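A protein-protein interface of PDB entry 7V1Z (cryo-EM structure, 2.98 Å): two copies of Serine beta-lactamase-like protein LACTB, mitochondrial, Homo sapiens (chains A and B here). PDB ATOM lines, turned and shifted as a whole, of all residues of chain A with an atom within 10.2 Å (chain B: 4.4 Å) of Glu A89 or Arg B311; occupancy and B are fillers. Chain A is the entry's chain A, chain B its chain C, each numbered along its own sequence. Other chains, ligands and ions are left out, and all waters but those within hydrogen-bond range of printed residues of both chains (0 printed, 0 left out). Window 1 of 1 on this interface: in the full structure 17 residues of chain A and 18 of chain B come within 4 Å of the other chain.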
ATOM      1  N   PRO A  65      29.723  -2.377  -9.356  1.00  0.00           N
ATOM      2  CA  PRO A  65      30.741  -2.913 -10.272  1.00  0.00           C
ATOM      3  C   PRO A  65      31.922  -1.982 -10.497  1.00  0.00           C
ATOM      4  O   PRO A  65      33.043  -2.467 -10.688  1.00  0.00           O
ATOM      5  CB  PRO A  65      29.957  -3.159 -11.570  1.00  0.00           C
ATOM      6  CG  PRO A  65      28.658  -2.441 -11.406  1.00  0.00           C
ATOM      7  CD  PRO A  65      28.377  -2.385  -9.948  1.00  0.00           C
ATOM      8  N   GLY A  84      37.272  -1.260 -10.779  1.00  0.00           N
ATOM      9  CA  GLY A  84      36.175  -2.068 -11.270  1.00  0.00           C
ATOM     10  C   GLY A  84      36.005  -2.029 -12.772  1.00  0.00           C
ATOM     11  O   GLY A  84      36.984  -1.904 -13.512  1.00  0.00           O
ATOM     12  N   TYR A  85      34.761  -2.137 -13.236  1.00  0.00           N
ATOM     13  CA  TYR A  85      34.454  -2.182 -14.658  1.00  0.00           C
ATOM     14  C   TYR A  85      33.350  -1.187 -14.975  1.00  0.00           C
ATOM     15  O   TYR A  85      32.311  -1.177 -14.310  1.00  0.00           O
ATOM     16  CB  TYR A  85      34.033  -3.591 -15.087  1.00  0.00           C
ATOM     17  CG  TYR A  85      35.143  -4.609 -14.993  1.00  0.00           C
ATOM     18  CD1 TYR A  85      35.393  -5.283 -13.807  1.00  0.00           C
ATOM     19  CD2 TYR A  85      35.947  -4.889 -16.087  1.00  0.00           C
ATOM     20  CE1 TYR A  85      36.410  -6.210 -13.715  1.00  0.00           C
ATOM     21  CE2 TYR A  85      36.966  -5.813 -16.005  1.00  0.00           C
ATOM     22  CZ  TYR A  85      37.193  -6.470 -14.817  1.00  0.00           C
ATOM     23  OH  TYR A  85      38.208  -7.394 -14.733  1.00  0.00           O
ATOM     24  N   ALA A  86      33.580  -0.351 -15.988  1.00  0.00           N
ATOM     25  CA  ALA A  86      32.539   0.557 -16.452  1.00  0.00           C
ATOM     26  C   ALA A  86      31.489  -0.177 -17.273  1.00  0.00           C
ATOM     27  O   ALA A  86      30.297   0.138 -17.188  1.00  0.00           O
ATOM     28  CB  ALA A  86      33.155   1.691 -17.270  1.00  0.00           C
ATOM     29  N   ASP A  87      31.913  -1.151 -18.074  1.00  0.00           N
ATOM     30  CA  ASP A  87      31.018  -1.996 -18.857  1.00  0.00           C
ATOM     31  C   ASP A  87      31.289  -3.442 -18.469  1.00  0.00           C
ATOM     32  O   ASP A  87      32.333  -4.000 -18.823  1.00  0.00           O
ATOM     33  CB  ASP A  87      31.223  -1.777 -20.355  1.00  0.00           C
ATOM     34  CG  ASP A  87      30.181  -2.487 -21.195  1.00  0.00           C
ATOM     35  OD1 ASP A  87      29.128  -2.869 -20.644  1.00  0.00           O
ATOM     36  OD2 ASP A  87      30.412  -2.660 -22.410  1.00  0.00           O
ATOM     37  N   VAL A  88      30.375  -4.067 -17.738  1.00  0.00           N
ATOM     38  CA  VAL A  88      30.591  -5.441 -17.278  1.00  0.00           C
ATOM     39  C   VAL A  88      30.568  -6.448 -18.424  1.00  0.00           C
ATOM     40  O   VAL A  88      31.405  -7.347 -18.480  1.00  0.00           O
ATOM     41  CB  VAL A  88      29.565  -5.834 -16.192  1.00  0.00           C
ATOM     42  CG1 VAL A  88      29.668  -7.311 -15.841  1.00  0.00           C
ATOM     43  CG2 VAL A  88      29.773  -4.984 -14.950  1.00  0.00           C
ATOM     44  N   GLU A  89      29.636  -6.288 -19.356  1.00  0.00           N
ATOM     45  CA  GLU A  89      29.505  -7.251 -20.450  1.00  0.00           C
ATOM     46  C   GLU A  89      30.729  -7.339 -21.354  1.00  0.00           C
ATOM     47  O   GLU A  89      31.131  -8.432 -21.745  1.00  0.00           O
ATOM     48  CB  GLU A  89      28.271  -6.917 -21.285  1.00  0.00           C
ATOM     49  CG  GLU A  89      26.987  -6.846 -20.476  1.00  0.00           C
ATOM     50  CD  GLU A  89      25.767  -6.584 -21.337  1.00  0.00           C
ATOM     51  OE1 GLU A  89      25.938  -6.250 -22.527  1.00  0.00           O
ATOM     52  OE2 GLU A  89      24.638  -6.712 -20.821  1.00  0.00           O
ATOM     53  N   ASN A  90      31.327  -6.200 -21.686  1.00  0.00           N
ATOM     54  CA  ASN A  90      32.478  -6.191 -22.589  1.00  0.00           C
ATOM     55  C   ASN A  90      33.810  -6.100 -21.861  1.00  0.00           C
ATOM     56  O   ASN A  90      34.843  -5.913 -22.503  1.00  0.00           O
ATOM     57  CB  ASN A  90      32.353  -5.076 -23.624  1.00  0.00           C
ATOM     58  CG  ASN A  90      31.218  -5.311 -24.599  1.00  0.00           C
ATOM     59  OD1 ASN A  90      30.559  -6.349 -24.564  1.00  0.00           O
ATOM     60  ND2 ASN A  90      30.985  -4.346 -25.480  1.00  0.00           N
ATOM     61  N   ARG A  91      33.793  -6.230 -20.538  1.00  0.00           N
ATOM     62  CA  ARG A  91      35.019  -6.168 -19.725  1.00  0.00           C
ATOM     63  C   ARG A  91      35.808  -4.875 -19.921  1.00  0.00           C
ATOM     64  O   ARG A  91      37.013  -4.919 -20.160  1.00  0.00           O
ATOM     65  CB  ARG A  91      35.916  -7.400 -19.939  1.00  0.00           C
ATOM     66  CG  ARG A  91      35.196  -8.745 -19.972  1.00  0.00           C
ATOM     67  CD  ARG A  91      34.264  -8.958 -18.789  1.00  0.00           C
ATOM     68  NE  ARG A  91      34.954  -8.980 -17.505  1.00  0.00           N
ATOM     69  CZ  ARG A  91      34.332  -9.050 -16.334  1.00  0.00           C
ATOM     70  NH1 ARG A  91      33.009  -9.097 -16.289  1.00  0.00           N
ATOM     71  NH2 ARG A  91      35.029  -9.068 -15.209  1.00  0.00           N
ATOM     72  N   VAL A  92      35.140  -3.731 -19.812  1.00  0.00           N
ATOM     73  CA  VAL A  92      35.787  -2.431 -19.968  1.00  0.00           C
ATOM     74  C   VAL A  92      36.106  -1.894 -18.577  1.00  0.00           C
ATOM     75  O   VAL A  92      35.175  -1.635 -17.800  1.00  0.00           O
ATOM     76  CB  VAL A  92      34.899  -1.447 -20.744  1.00  0.00           C
ATOM     77  CG1 VAL A  92      35.587  -0.104 -20.869  1.00  0.00           C
ATOM     78  CG2 VAL A  92      34.566  -2.004 -22.114  1.00  0.00           C
ATOM     79  N   PRO A  93      37.374  -1.713 -18.224  1.00  0.00           N
ATOM     80  CA  PRO A  93      37.705  -1.212 -16.886  1.00  0.00           C
ATOM     81  C   PRO A  93      37.379   0.266 -16.737  1.00  0.00           C
ATOM     82  O   PRO A  93      37.213   1.002 -17.712  1.00  0.00           O
ATOM     83  CB  PRO A  93      39.211  -1.461 -16.774  1.00  0.00           C
ATOM     84  CG  PRO A  93      39.692  -1.486 -18.178  1.00  0.00           C
ATOM     85  CD  PRO A  93      38.576  -2.055 -19.002  1.00  0.00           C
ATOM     86  N   ALA A 312      29.857   4.934 -19.845  1.00  0.00           N
ATOM     87  CA  ALA A 312      29.684   3.779 -18.966  1.00  0.00           C
ATOM     88  C   ALA A 312      28.276   3.213 -18.997  1.00  0.00           C
ATOM     89  O   ALA A 312      27.353   3.850 -19.502  1.00  0.00           O
ATOM     90  CB  ALA A 312      30.061   4.142 -17.541  1.00  0.00           C
ATOM     91  N   ARG A 313      28.103   2.014 -18.449  1.00  0.00           N
ATOM     92  CA  ARG A 313      26.781   1.400 -18.396  1.00  0.00           C
ATOM     93  C   ARG A 313      26.263   1.404 -16.972  1.00  0.00           C
ATOM     94  O   ARG A 313      27.050   1.388 -16.030  1.00  0.00           O
ATOM     95  CB  ARG A 313      26.824  -0.014 -18.957  1.00  0.00           C
ATOM     96  CG  ARG A 313      27.211  -0.078 -20.421  1.00  0.00           C
ATOM     97  CD  ARG A 313      25.997  -0.337 -21.292  1.00  0.00           C
ATOM     98  NE  ARG A 313      25.502  -1.703 -21.153  1.00  0.00           N
ATOM     99  CZ  ARG A 313      24.523  -2.216 -21.891  1.00  0.00           C
ATOM    100  NH1 ARG A 313      23.935  -1.474 -22.819  1.00  0.00           N
ATOM    101  NH2 ARG A 313      24.132  -3.468 -21.702  1.00  0.00           N
ATOM    102  N   PHE A 314      24.946   1.415 -16.801  1.00  0.00           N
ATOM    103  CA  PHE A 314      24.369   1.528 -15.458  1.00  0.00           C
ATOM    104  C   PHE A 314      23.624   0.263 -15.066  1.00  0.00           C
ATOM    105  O   PHE A 314      22.913  -0.303 -15.896  1.00  0.00           O
ATOM    106  CB  PHE A 314      23.549   2.816 -15.390  1.00  0.00           C
ATOM    107  CG  PHE A 314      24.318   4.013 -15.885  1.00  0.00           C
ATOM    108  CD1 PHE A 314      25.363   4.530 -15.136  1.00  0.00           C
ATOM    109  CD2 PHE A 314      24.057   4.568 -17.127  1.00  0.00           C
ATOM    110  CE1 PHE A 314      26.103   5.603 -15.594  1.00  0.00           C
ATOM    111  CE2 PHE A 314      24.796   5.638 -17.593  1.00  0.00           C
ATOM    112  CZ  PHE A 314      25.819   6.157 -16.824  1.00  0.00           C
ATOM    113  N   TYR A 315      23.761  -0.187 -13.814  1.00  0.00           N
ATOM    114  CA  TYR A 315      23.216  -1.482 -13.437  1.00  0.00           C
ATOM    115  C   TYR A 315      22.384  -1.363 -12.165  1.00  0.00           C
ATOM    116  O   TYR A 315      22.364  -0.326 -11.499  1.00  0.00           O
ATOM    117  CB  TYR A 315      24.337  -2.507 -13.237  1.00  0.00           C
ATOM    118  CG  TYR A 315      25.257  -2.640 -14.427  1.00  0.00           C
ATOM    119  CD1 TYR A 315      24.836  -3.274 -15.586  1.00  0.00           C
ATOM    120  CD2 TYR A 315      26.548  -2.132 -14.391  1.00  0.00           C
ATOM    121  CE1 TYR A 315      25.672  -3.398 -16.672  1.00  0.00           C
ATOM    122  CE2 TYR A 315      27.390  -2.252 -15.475  1.00  0.00           C
ATOM    123  CZ  TYR A 315      26.947  -2.887 -16.614  1.00  0.00           C
ATOM    124  OH  TYR A 315      27.781  -3.010 -17.699  1.00  0.00           O
ATOM    125  N   LEU A 323      22.998  -9.014 -10.650  1.00  0.00           N
ATOM    126  CA  LEU A 323      23.158  -7.738 -11.342  1.00  0.00           C
ATOM    127  C   LEU A 323      22.472  -7.730 -12.702  1.00  0.00           C
ATOM    128  O   LEU A 323      22.605  -8.685 -13.462  1.00  0.00           O
ATOM    129  CB  LEU A 323      24.643  -7.440 -11.523  1.00  0.00           C
ATOM    130  CG  LEU A 323      25.021  -5.988 -11.788  1.00  0.00           C
ATOM    131  CD1 LEU A 323      24.605  -5.142 -10.598  1.00  0.00           C
ATOM    132  CD2 LEU A 323      26.516  -5.874 -12.036  1.00  0.00           C
ATOM    133  N   VAL A 324      21.762  -6.649 -13.021  1.00  0.00           N
ATOM    134  CA  VAL A 324      21.077  -6.534 -14.313  1.00  0.00           C
ATOM    135  C   VAL A 324      21.134  -5.117 -14.880  1.00  0.00           C
ATOM    136  O   VAL A 324      21.468  -4.182 -14.164  1.00  0.00           O
ATOM    137  CB  VAL A 324      19.592  -6.972 -14.239  1.00  0.00           C
ATOM    138  CG1 VAL A 324      19.448  -8.485 -14.277  1.00  0.00           C
ATOM    139  CG2 VAL A 324      18.892  -6.379 -13.030  1.00  0.00           C
ATOM    140  N   ASN A 325      20.804  -4.951 -16.160  1.00  0.00           N
ATOM    141  CA  ASN A 325      20.791  -3.639 -16.787  1.00  0.00           C
ATOM    142  C   ASN A 325      19.523  -2.886 -16.412  1.00  0.00           C
ATOM    143  O   ASN A 325      18.449  -3.478 -16.282  1.00  0.00           O
ATOM    144  CB  ASN A 325      20.875  -3.768 -18.308  1.00  0.00           C
ATOM    145  CG  ASN A 325      22.240  -4.210 -18.782  1.00  0.00           C
ATOM    146  OD1 ASN A 325      23.234  -3.514 -18.582  1.00  0.00           O
ATOM    147  ND2 ASN A 325      22.295  -5.369 -19.421  1.00  0.00           N
ATOM    148  N   THR A 326      19.655  -1.579 -16.234  1.00  0.00           N
ATOM    149  CA  THR A 326      18.488  -0.747 -16.004  1.00  0.00           C
ATOM    150  C   THR A 326      17.743  -0.513 -17.318  1.00  0.00           C
ATOM    151  O   THR A 326      18.337  -0.588 -18.397  1.00  0.00           O
ATOM    152  CB  THR A 326      18.896   0.589 -15.395  1.00  0.00           C
ATOM    153  OG1 THR A 326      19.733   1.300 -16.315  1.00  0.00           O
ATOM    154  CG2 THR A 326      19.657   0.369 -14.102  1.00  0.00           C
ATOM    155  N   ASN A 464      28.500   3.568 -10.732  1.00  0.00           N
ATOM    156  CA  ASN A 464      27.408   3.104 -11.589  1.00  0.00           C
ATOM    157  C   ASN A 464      26.551   2.063 -10.868  1.00  0.00           C
ATOM    158  O   ASN A 464      26.298   0.967 -11.360  1.00  0.00           O
ATOM    159  CB  ASN A 464      27.963   2.557 -12.900  1.00  0.00           C
ATOM    160  CG  ASN A 464      29.049   1.520 -12.689  1.00  0.00           C
ATOM    161  OD1 ASN A 464      29.391   1.185 -11.557  1.00  0.00           O
ATOM    162  ND2 ASN A 464      29.595   1.007 -13.783  1.00  0.00           N
ATOM    163  N   VAL B  99      28.823 -11.347 -30.074  1.00  0.00           N
ATOM    164  CA  VAL B  99      27.415 -11.705 -30.193  1.00  0.00           C
ATOM    165  C   VAL B  99      26.705 -10.586 -30.942  1.00  0.00           C
ATOM    166  O   VAL B  99      26.714  -9.432 -30.499  1.00  0.00           O
ATOM    167  CB  VAL B  99      26.778 -11.944 -28.815  1.00  0.00           C
ATOM    168  CG1 VAL B  99      25.270 -11.883 -28.907  1.00  0.00           C
ATOM    169  CG2 VAL B  99      27.223 -13.280 -28.254  1.00  0.00           C
ATOM    170  N   GLU B 303      17.138  -9.491 -25.057  1.00  0.00           N
ATOM    171  CA  GLU B 303      16.431  -8.702 -24.061  1.00  0.00           C
ATOM    172  C   GLU B 303      17.422  -7.773 -23.378  1.00  0.00           C
ATOM    173  O   GLU B 303      18.603  -8.098 -23.235  1.00  0.00           O
ATOM    174  CB  GLU B 303      15.731  -9.589 -23.027  1.00  0.00           C
ATOM    175  CG  GLU B 303      14.368 -10.095 -23.464  1.00  0.00           C
ATOM    176  CD  GLU B 303      14.015 -11.426 -22.834  1.00  0.00           C
ATOM    177  OE1 GLU B 303      12.816 -11.667 -22.584  1.00  0.00           O
ATOM    178  OE2 GLU B 303      14.936 -12.231 -22.586  1.00  0.00           O
ATOM    179  N   ASN B 304      16.930  -6.607 -22.958  1.00  0.00           N
ATOM    180  CA  ASN B 304      17.810  -5.597 -22.379  1.00  0.00           C
ATOM    181  C   ASN B 304      18.216  -5.957 -20.955  1.00  0.00           C
ATOM    182  O   ASN B 304      19.373  -5.765 -20.563  1.00  0.00           O
ATOM    183  CB  ASN B 304      17.131  -4.230 -22.416  1.00  0.00           C
ATOM    184  CG  ASN B 304      18.079  -3.100 -22.073  1.00  0.00           C
ATOM    185  OD1 ASN B 304      19.260  -3.143 -22.413  1.00  0.00           O
ATOM    186  ND2 ASN B 304      17.564  -2.080 -21.399  1.00  0.00           N
ATOM    187  N   PRO B 306      18.652  -8.887 -19.015  1.00  0.00           N
ATOM    188  CA  PRO B 306      19.704  -9.844 -18.648  1.00  0.00           C
ATOM    189  C   PRO B 306      21.077  -9.386 -19.117  1.00  0.00           C
ATOM    190  O   PRO B 306      21.210  -8.661 -20.105  1.00  0.00           O
ATOM    191  CB  PRO B 306      19.276 -11.134 -19.356  1.00  0.00           C
ATOM    192  CG  PRO B 306      18.413 -10.683 -20.467  1.00  0.00           C
ATOM    193  CD  PRO B 306      17.680  -9.497 -19.940  1.00  0.00           C
ATOM    194  N   VAL B 307      22.103  -9.821 -18.390  1.00  0.00           N
ATOM    195  CA  VAL B 307      23.485  -9.524 -18.749  1.00  0.00           C
ATOM    196  C   VAL B 307      23.943 -10.561 -19.770  1.00  0.00           C
ATOM    197  O   VAL B 307      23.973 -11.759 -19.481  1.00  0.00           O
ATOM    198  CB  VAL B 307      24.397  -9.516 -17.518  1.00  0.00           C
ATOM    199  CG1 VAL B 307      25.856  -9.567 -17.937  1.00  0.00           C
ATOM    200  CG2 VAL B 307      24.130  -8.283 -16.675  1.00  0.00           C
ATOM    201  N   ILE B 308      24.299 -10.100 -20.965  1.00  0.00           N
ATOM    202  CA  ILE B 308      24.783 -10.959 -22.041  1.00  0.00           C
ATOM    203  C   ILE B 308      26.213 -10.550 -22.355  1.00  0.00           C
ATOM    204  O   ILE B 308      26.465  -9.406 -22.752  1.00  0.00           O
ATOM    205  CB  ILE B 308      23.891 -10.860 -23.287  1.00  0.00           C
ATOM    206  CG1 ILE B 308      22.462 -11.282 -22.948  1.00  0.00           C
ATOM    207  CG2 ILE B 308      24.452 -11.710 -24.409  1.00  0.00           C
ATOM    208  CD1 ILE B 308      21.521 -11.245 -24.122  1.00  0.00           C
ATOM    209  N   TYR B 309      27.145 -11.481 -22.189  1.00  0.00           N
ATOM    210  CA  TYR B 309      28.554 -11.156 -22.332  1.00  0.00           C
ATOM    211  C   TYR B 309      28.948 -11.036 -23.800  1.00  0.00           C
ATOM    212  O   TYR B 309      28.399 -11.711 -24.675  1.00  0.00           O
ATOM    213  CB  TYR B 309      29.414 -12.210 -21.638  1.00  0.00           C
ATOM    214  CG  TYR B 309      29.359 -12.111 -20.135  1.00  0.00           C
ATOM    215  CD1 TYR B 309      28.387 -12.786 -19.411  1.00  0.00           C
ATOM    216  CD2 TYR B 309      30.269 -11.328 -19.438  1.00  0.00           C
ATOM    217  CE1 TYR B 309      28.328 -12.692 -18.037  1.00  0.00           C
ATOM    218  CE2 TYR B 309      30.217 -11.229 -18.064  1.00  0.00           C
ATOM    219  CZ  TYR B 309      29.246 -11.913 -17.368  1.00  0.00           C
ATOM    220  OH  TYR B 309      29.192 -11.816 -15.998  1.00  0.00           O
ATOM    221  N   ASN B 310      29.917 -10.163 -24.078  1.00  0.00           N
ATOM    222  CA  ASN B 310      30.401  -9.957 -25.453  1.00  0.00           C
ATOM    223  C   ASN B 310      29.340  -9.474 -26.433  1.00  0.00           C
ATOM    224  O   ASN B 310      29.444  -9.725 -27.630  1.00  0.00           O
ATOM    225  CB  ASN B 310      31.126 -11.199 -25.981  1.00  0.00           C
ATOM    226  CG  ASN B 310      32.282 -11.618 -25.095  1.00  0.00           C
ATOM    227  OD1 ASN B 310      32.839 -10.806 -24.357  1.00  0.00           O
ATOM    228  ND2 ASN B 310      32.649 -12.891 -25.162  1.00  0.00           N
ATOM    229  N   ARG B 311      28.335  -8.757 -25.936  1.00  0.00           N
ATOM    230  CA  ARG B 311      27.299  -8.206 -26.809  1.00  0.00           C
ATOM    231  C   ARG B 311      27.869  -7.041 -27.615  1.00  0.00           C
ATOM    232  O   ARG B 311      28.750  -6.333 -27.131  1.00  0.00           O
ATOM    233  CB  ARG B 311      26.082  -7.782 -25.986  1.00  0.00           C
ATOM    234  CG  ARG B 311      24.852  -7.434 -26.807  1.00  0.00           C
ATOM    235  CD  ARG B 311      23.566  -7.714 -26.048  1.00  0.00           C
ATOM    236  NE  ARG B 311      23.510  -7.041 -24.754  1.00  0.00           N
ATOM    237  CZ  ARG B 311      22.446  -7.050 -23.959  1.00  0.00           C
ATOM    238  NH1 ARG B 311      21.345  -7.689 -24.331  1.00  0.00           N
ATOM    239  NH2 ARG B 311      22.474  -6.414 -22.796  1.00  0.00           N
ATOM    240  N   ALA B 312      27.378  -6.827 -28.835  1.00  0.00           N
ATOM    241  CA  ALA B 312      27.943  -5.792 -29.704  1.00  0.00           C
ATOM    242  C   ALA B 312      26.962  -4.679 -30.020  1.00  0.00           C
ATOM    243  O   ALA B 312      25.753  -4.868 -29.927  1.00  0.00           O
ATOM    244  CB  ALA B 312      28.444  -6.410 -30.995  1.00  0.00           C
ATOM    245  N   LEU B 341      19.990 -13.661 -30.832  1.00  0.00           N
ATOM    246  CA  LEU B 341      21.407 -13.335 -30.814  1.00  0.00           C
ATOM    247  C   LEU B 341      22.209 -14.618 -30.960  1.00  0.00           C
ATOM    248  O   LEU B 341      21.791 -15.680 -30.497  1.00  0.00           O
ATOM    249  CB  LEU B 341      21.810 -12.614 -29.524  1.00  0.00           C
ATOM    250  CG  LEU B 341      21.142 -11.274 -29.218  1.00  0.00           C
ATOM    251  CD1 LEU B 341      21.450 -10.852 -27.797  1.00  0.00           C
ATOM    252  CD2 LEU B 341      21.591 -10.209 -30.197  1.00  0.00           C
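The backbone carbonyl oxygen (O) of Asn B304 is in hydrogen-bond range of the side-chain amide nitrogen (ND2) of Asn A325. The side-chain carboxylate (OE2) of Glu A89 is in salt-bridge range of the guanidinium group (NH2) of Arg B311, 2.9 Å away. The backbone carbonyl oxygen of Arg B311 lies close to the side-chain amide oxygen of Asn A90 (3.1 Å). O of Glu A89 sits at hydrogen-bond distance from N of Asn B310 (3.1 Å). O of Thr A326 sits at hydrogen-bond distance from ND2 of Asn B304 (3.4 Å). The backbone NH (N) of Ile B308 lies within hydrogen-bond range of the side-chain carboxylate (OE2) of Glu A89 (3.4 Å).
The guanidinium group (NH1) of Arg A91 lies within hydrogen-bond range of the backbone carbonyl oxygen (O) of Val A88, at 3.2 Å. ND2 of Asn A325 is in hydrogen-bond range of OE2 of Glu A89, at 3.0 Å. The backbone carbonyl oxygen of Glu B303 is in hydrogen-bond range of the guanidinium group of Arg B311 (3.0 Å). The backbone carbonyl oxygen (O) of Arg A313 lies within hydrogen-bond range of the side-chain amide nitrogen (ND2) of Asn A464 (3.4 Å). The backbone carbonyl oxygen (O) of Ala A86 is in hydrogen-bond range of the backbone NH (N) of Arg A313 (3.2 Å). The backbone NH of Val B99 is in hydrogen-bond range of the backbone carbonyl oxygen of Asn B310.
OE2 of Glu A89 touches CA of Val B307, 3.7 Å away. Tyr B309 touches Glu A89. Asn A90 touches Asn B310. CE2 of Tyr B309 touches NH1 of Arg A91, at 3.9 Å. Arg A313 touches Arg B311. O of Leu A323 touches CG2 of Val B307, 3.6 Å away. ND2 of Asn A325 touches O of Pro B306 (3.5 Å). ND2 of Asn A325 touches NH2 of Arg B311 (3.5 Å).
Gly A84 touches none of the printed residues of chain B. Printed residues of chain B within 4 Å of Arg A91: Tyr B309 (3.9 Å). Of the printed residues of chain B, Thr A326 touches Asn B304. No residue of chain A comes within 4 Å of Val B99. Ile B308 touches just one residue of chain A: Glu A89 (3.2 Å). Of the printed residues of chain A, Tyr B309 touches Glu A89 (3.8 Å) and Arg A91 (3.9 Å). Of chain A, only Glu A89 (3.1 Å) and Asn A90 (3.7 Å) come within 4 Å of Asn B310. No residue of chain A comes within 4 Å of Ala B312. The nearest printed residue of chain B that does not touch Glu A89 is Pro B306 (4.01 Å). The nearest residue of chain A that does not touch Arg B311 is Asp A87 (6.2 Å). The nearest printed residue of chain A that does not touch Tyr B309 is Val A88 (4.1 Å).
Along chain A the printed residues that touch a printed residue of chain B span positions 89 to 326. Hydrophobic or aromatic side chains of chain B that line the printed part of chain A: Val B307 and Tyr B309. Among the printed residues, Asp or Glu carboxylates within 4 Å of a Lys or Arg side-chain nitrogen of the other chain: Glu A89 with Arg B311 (2.9 Å).
1 position is printed for both chains.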
